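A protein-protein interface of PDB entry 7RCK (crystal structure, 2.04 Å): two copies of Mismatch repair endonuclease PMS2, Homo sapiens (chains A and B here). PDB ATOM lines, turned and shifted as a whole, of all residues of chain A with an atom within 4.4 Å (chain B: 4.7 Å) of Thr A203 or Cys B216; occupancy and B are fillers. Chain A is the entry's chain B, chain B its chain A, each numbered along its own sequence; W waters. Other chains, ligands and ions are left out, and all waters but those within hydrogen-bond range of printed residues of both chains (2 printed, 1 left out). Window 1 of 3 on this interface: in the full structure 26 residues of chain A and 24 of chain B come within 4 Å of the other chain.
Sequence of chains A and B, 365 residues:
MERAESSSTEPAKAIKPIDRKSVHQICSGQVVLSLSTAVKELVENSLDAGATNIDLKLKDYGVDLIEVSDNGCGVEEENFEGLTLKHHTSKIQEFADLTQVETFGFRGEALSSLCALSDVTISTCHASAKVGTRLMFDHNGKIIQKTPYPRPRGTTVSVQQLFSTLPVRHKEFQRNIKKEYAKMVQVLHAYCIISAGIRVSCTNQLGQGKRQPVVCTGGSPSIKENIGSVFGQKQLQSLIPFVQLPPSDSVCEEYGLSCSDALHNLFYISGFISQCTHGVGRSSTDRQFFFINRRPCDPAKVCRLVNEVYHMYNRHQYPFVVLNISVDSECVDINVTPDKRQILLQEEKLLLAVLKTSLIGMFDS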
ATOM      1  N   LEU A  56      -7.338  28.379  22.847  1.00  0.00           N
ATOM      2  CA  LEU A  56      -6.048  29.050  22.778  1.00  0.00           C
ATOM      3  C   LEU A  56      -5.198  28.321  21.748  1.00  0.00           C
ATOM      4  O   LEU A  56      -4.866  27.145  21.932  1.00  0.00           O
ATOM      5  CB  LEU A  56      -5.367  29.057  24.147  1.00  0.00           C
ATOM      6  CG  LEU A  56      -3.914  29.533  24.232  1.00  0.00           C
ATOM      7  CD1 LEU A  56      -3.780  30.974  23.756  1.00  0.00           C
ATOM      8  CD2 LEU A  56      -3.386  29.379  25.652  1.00  0.00           C
ATOM      9  N   LYS A  57      -4.850  29.015  20.669  1.00  0.00           N
ATOM     10  CA  LYS A  57      -4.058  28.447  19.586  1.00  0.00           C
ATOM     11  C   LYS A  57      -2.673  29.074  19.615  1.00  0.00           C
ATOM     12  O   LYS A  57      -2.541  30.299  19.524  1.00  0.00           O
ATOM     13  CB  LYS A  57      -4.730  28.679  18.232  1.00  0.00           C
ATOM     14  CG  LYS A  57      -3.940  28.137  17.053  1.00  0.00           C
ATOM     15  CD  LYS A  57      -4.463  28.664  15.724  1.00  0.00           C
ATOM     16  CE  LYS A  57      -5.823  28.085  15.391  1.00  0.00           C
ATOM     17  NZ  LYS A  57      -6.318  28.562  14.067  1.00  0.00           N
ATOM     18  N   LEU A  58      -1.650  28.235  19.742  1.00  0.00           N
ATOM     19  CA  LEU A  58      -0.269  28.685  19.816  1.00  0.00           C
ATOM     20  C   LEU A  58       0.527  28.149  18.634  1.00  0.00           C
ATOM     21  O   LEU A  58       0.288  27.037  18.151  1.00  0.00           O
ATOM     22  CB  LEU A  58       0.401  28.230  21.120  1.00  0.00           C
ATOM     23  CG  LEU A  58      -0.235  28.648  22.445  1.00  0.00           C
ATOM     24  CD1 LEU A  58       0.367  27.842  23.587  1.00  0.00           C
ATOM     25  CD2 LEU A  58      -0.059  30.139  22.687  1.00  0.00           C
ATOM     26  N   CYS A 202      -6.460  24.203  24.459  1.00  0.00           N
ATOM     27  CA  CYS A 202      -5.206  24.769  23.992  1.00  0.00           C
ATOM     28  C   CYS A 202      -4.555  23.805  23.014  1.00  0.00           C
ATOM     29  O   CYS A 202      -4.546  22.591  23.238  1.00  0.00           O
ATOM     30  CB  CYS A 202      -4.245  25.058  25.150  1.00  0.00           C
ATOM     31  SG  CYS A 202      -2.625  25.664  24.631  1.00  0.00           S
ATOM     32  N   THR A 203      -4.029  24.353  21.920  1.00  0.00           N
ATOM     33  CA  THR A 203      -3.265  23.595  20.944  1.00  0.00           C
ATOM     34  C   THR A 203      -1.970  24.334  20.648  1.00  0.00           C
ATOM     35  O   THR A 203      -1.885  25.554  20.808  1.00  0.00           O
ATOM     36  CB  THR A 203      -4.042  23.390  19.636  1.00  0.00           C
ATOM     37  OG1 THR A 203      -4.213  24.655  18.984  1.00  0.00           O
ATOM     38  CG2 THR A 203      -5.407  22.771  19.906  1.00  0.00           C
ATOM     39  N   ASN A 204      -0.961  23.585  20.212  1.00  0.00           N
ATOM     40  CA  ASN A 204       0.334  24.159  19.879  1.00  0.00           C
ATOM     41  C   ASN A 204       0.870  23.501  18.616  1.00  0.00           C
ATOM     42  O   ASN A 204       0.668  22.302  18.401  1.00  0.00           O
ATOM     43  CB  ASN A 204       1.319  24.001  21.045  1.00  0.00           C
ATOM     44  CG  ASN A 204       2.624  24.732  20.813  1.00  0.00           C
ATOM     45  OD1 ASN A 204       2.672  25.734  20.099  1.00  0.00           O
ATOM     46  ND2 ASN A 204       3.690  24.251  21.444  1.00  0.00           N
ATOM     47  N   ARG A 211      -0.402  20.340  13.991  1.00  0.00           N
ATOM     48  CA  ARG A 211      -0.975  20.941  15.186  1.00  0.00           C
ATOM     49  C   ARG A 211      -1.300  19.853  16.204  1.00  0.00           C
ATOM     50  O   ARG A 211      -1.850  18.803  15.860  1.00  0.00           O
ATOM     51  CB  ARG A 211      -2.227  21.743  14.838  1.00  0.00           C
ATOM     52  CG  ARG A 211      -2.789  22.503  16.022  1.00  0.00           C
ATOM     53  CD  ARG A 211      -3.691  23.645  15.603  1.00  0.00           C
ATOM     54  NE  ARG A 211      -2.908  24.760  15.086  1.00  0.00           N
ATOM     55  CZ  ARG A 211      -2.127  25.532  15.830  1.00  0.00           C
ATOM     56  NH1 ARG A 211      -2.004  25.343  17.136  1.00  0.00           N
ATOM     57  NH2 ARG A 211      -1.446  26.516  15.249  1.00  0.00           N
ATOM     58  N   GLN A 212      -0.949  20.101  17.463  1.00  0.00           N
ATOM     59  CA  GLN A 212      -1.126  19.104  18.502  1.00  0.00           C
ATOM     60  C   GLN A 212      -1.997  19.627  19.638  1.00  0.00           C
ATOM     61  O   GLN A 212      -1.781  20.750  20.114  1.00  0.00           O
ATOM     62  CB  GLN A 212       0.238  18.656  19.047  1.00  0.00           C
ATOM     63  CG  GLN A 212       1.093  17.977  17.986  1.00  0.00           C
ATOM     64  CD  GLN A 212       2.107  17.017  18.565  1.00  0.00           C
ATOM     65  OE1 GLN A 212       2.209  15.871  18.128  1.00  0.00           O
ATOM     66  NE2 GLN A 212       2.869  17.480  19.550  1.00  0.00           N
ATOM     67  N   PRO A 213      -2.984  18.857  20.094  1.00  0.00           N
ATOM     68  CA  PRO A 213      -3.762  19.277  21.265  1.00  0.00           C
ATOM     69  C   PRO A 213      -2.900  19.263  22.519  1.00  0.00           C
ATOM     70  O   PRO A 213      -2.044  18.394  22.698  1.00  0.00           O
ATOM     71  CB  PRO A 213      -4.891  18.242  21.337  1.00  0.00           C
ATOM     72  CG  PRO A 213      -4.372  17.055  20.596  1.00  0.00           C
ATOM     73  CD  PRO A 213      -3.489  17.600  19.515  1.00  0.00           C
ATOM     74  N   VAL A 214      -3.120  20.252  23.380  1.00  0.00           N
ATOM     75  CA  VAL A 214      -2.404  20.385  24.644  1.00  0.00           C
ATOM     76  C   VAL A 214      -3.297  20.038  25.829  1.00  0.00           C
ATOM     77  O   VAL A 214      -2.900  19.282  26.716  1.00  0.00           O
ATOM     78  CB  VAL A 214      -1.806  21.804  24.796  1.00  0.00           C
ATOM     79  CG1 VAL A 214      -1.148  21.962  26.159  1.00  0.00           C
ATOM     80  CG2 VAL A 214      -0.809  22.083  23.682  1.00  0.00           C
ATOM     81  N   VAL B 200     -11.705  20.238  15.019  1.00  0.00           N
ATOM     82  CA  VAL B 200     -11.785  18.832  15.390  1.00  0.00           C
ATOM     83  C   VAL B 200     -10.467  18.454  16.045  1.00  0.00           C
ATOM     84  O   VAL B 200      -9.399  18.740  15.496  1.00  0.00           O
ATOM     85  CB  VAL B 200     -12.069  17.937  14.171  1.00  0.00           C
ATOM     86  CG1 VAL B 200     -12.195  16.479  14.598  1.00  0.00           C
ATOM     87  CG2 VAL B 200     -13.324  18.405  13.451  1.00  0.00           C
ATOM     88  N   SER B 201     -10.537  17.821  17.215  1.00  0.00           N
ATOM     89  CA  SER B 201      -9.340  17.391  17.922  1.00  0.00           C
ATOM     90  C   SER B 201      -9.553  15.977  18.441  1.00  0.00           C
ATOM     91  O   SER B 201     -10.685  15.550  18.679  1.00  0.00           O
ATOM     92  CB  SER B 201      -8.988  18.337  19.079  1.00  0.00           C
ATOM     93  OG  SER B 201      -9.941  18.249  20.125  1.00  0.00           O
ATOM     94  N   VAL B 215      -4.692  14.183  16.425  1.00  0.00           N
ATOM     95  CA  VAL B 215      -4.900  15.160  15.363  1.00  0.00           C
ATOM     96  C   VAL B 215      -5.706  16.322  15.929  1.00  0.00           C
ATOM     97  O   VAL B 215      -6.446  16.156  16.906  1.00  0.00           O
ATOM     98  CB  VAL B 215      -5.610  14.533  14.146  1.00  0.00           C
ATOM     99  CG1 VAL B 215      -7.067  14.255  14.466  1.00  0.00           C
ATOM    100  CG2 VAL B 215      -5.481  15.429  12.922  1.00  0.00           C
ATOM    101  N   CYS B 216      -5.539  17.512  15.354  1.00  0.00           N
ATOM    102  CA  CYS B 216      -6.419  18.628  15.666  1.00  0.00           C
ATOM    103  C   CYS B 216      -6.312  19.678  14.567  1.00  0.00           C
ATOM    104  O   CYS B 216      -5.215  19.968  14.083  1.00  0.00           O
ATOM    105  CB  CYS B 216      -6.122  19.238  17.039  1.00  0.00           C
ATOM    106  SG  CYS B 216      -4.510  19.955  17.230  1.00  0.00           S
ATOM    107  N   THR B 217      -7.457  20.212  14.158  1.00  0.00           N
ATOM    108  CA  THR B 217      -7.527  21.305  13.199  1.00  0.00           C
ATOM    109  C   THR B 217      -7.775  22.623  13.925  1.00  0.00           C
ATOM    110  O   THR B 217      -8.271  22.652  15.053  1.00  0.00           O
ATOM    111  CB  THR B 217      -8.625  21.051  12.159  1.00  0.00           C
ATOM    112  OG1 THR B 217      -9.873  20.809  12.822  1.00  0.00           O
ATOM    113  CG2 THR B 217      -8.277  19.844  11.305  1.00  0.00           C
ATOM    114  N   GLY B 218      -7.415  23.720  13.265  1.00  0.00           N
ATOM    115  CA  GLY B 218      -7.446  25.034  13.874  1.00  0.00           C
ATOM    116  C   GLY B 218      -8.655  25.890  13.564  1.00  0.00           C
ATOM    117  O   GLY B 218      -8.621  27.100  13.828  1.00  0.00           O
ATOM    118  N   SER B 229      -2.680  21.514   9.192  1.00  0.00           N
ATOM    119  CA  SER B 229      -2.869  21.189  10.603  1.00  0.00           C
ATOM    120  C   SER B 229      -2.755  19.688  10.850  1.00  0.00           C
ATOM    121  O   SER B 229      -2.213  19.262  11.878  1.00  0.00           O
ATOM    122  CB  SER B 229      -4.221  21.707  11.088  1.00  0.00           C
ATOM    123  OG  SER B 229      -4.256  23.123  11.083  1.00  0.00           O
HETATM  124  O   HOH W   1      -2.834  17.440  13.816  1.00  0.00           O
HETATM  125  O   HOH W   2      -2.967  25.131  12.638  1.00  0.00           O
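The side-chain sulfur (SG) of Cys B216 lies close to the backbone NH (N) of Gln A212 (3.6 Å). O of Arg A211 is in hydrogen-bond range of SG of Cys B216, at 3.2 Å. The backbone carbonyl oxygen (O) of Ser B229 sits at hydrogen-bond distance from the backbone NH (N) of Arg A211, at 3.0 Å. The side-chain sulfur (SG) of Cys B216 sits close to the backbone nitrogen (N) of Pro A213. O of Gly B218 lies within hydrogen-bond range of NZ of Lys A57 (2.7 Å).
Water W2 lies within hydrogen-bond range of the guanidinium group (NE) of Arg A211 (2.5 Å) and the side-chain hydroxyl (OG) of Ser B229 (2.8 Å). Water W1 lies within hydrogen-bond range of the backbone carbonyl oxygen (O) of Arg A211 (2.6 Å), the backbone carbonyl oxygen (O) of Ser B229 (2.7 Å) and the backbone NH (N) of Cys B216 (3.1 Å).
The side-chain hydroxyl (OG1) of Thr A203 sits at hydrogen-bond distance from the guanidinium group (NH1) of Arg A211, at 3.0 Å. O of Leu A58 is in hydrogen-bond range of NH1 of Arg A211 (3.0 Å). O of Leu A56 sits at hydrogen-bond distance from N of Thr A203 (2.9 Å). The backbone carbonyl oxygen of Asn A204 lies within hydrogen-bond range of the backbone NH of Gln A212, 2.9 Å away. The backbone NH (N) of Leu A58 sits at hydrogen-bond distance from the backbone carbonyl oxygen (O) of Thr A203 (2.9 Å).
Printed residues of chain A that touch a printed residue of chain B: Lys A57, Thr A203, Arg A211, Gln A212 and Pro A213. Hydrophobic or aromatic side chains of chain A that line the printed part of chain B: Pro A213. Among the printed residues, no Asp or Glu carboxylate lies within 4 Å of a Lys or Arg side-chain nitrogen of the other chain.
Among the printed residues, merely in contact across the chains: Thr A203 with Cys B216 (3.99 Å).
Printed residues of chain A within 4 Å of Cys B216: Thr A203, Arg A211, Gln A212 and Pro A213. Of the printed residues of chain B, Lys A57 touches Gly B218. Printed residues of chain A within 4 Å of Gly B218: Lys A57 (2.7 Å). Leu A58 touches none of the printed residues of chain B. Val B200 touches none of the printed residues of chain A. The nearest printed residue of chain B that does not touch Thr A203 is Thr B217 (5.6 Å). The nearest printed residue of chain A that does not touch Cys B216 is Asn A204 (5.8 Å). The nearest printed residue of chain B that does not touch Lys A57 is Thr B217 (6.0 Å).
No position is printed for both chains. Of the 6 pairs that touch across the chains among the printed residues, none has its exchanged pair printed and touching as well.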
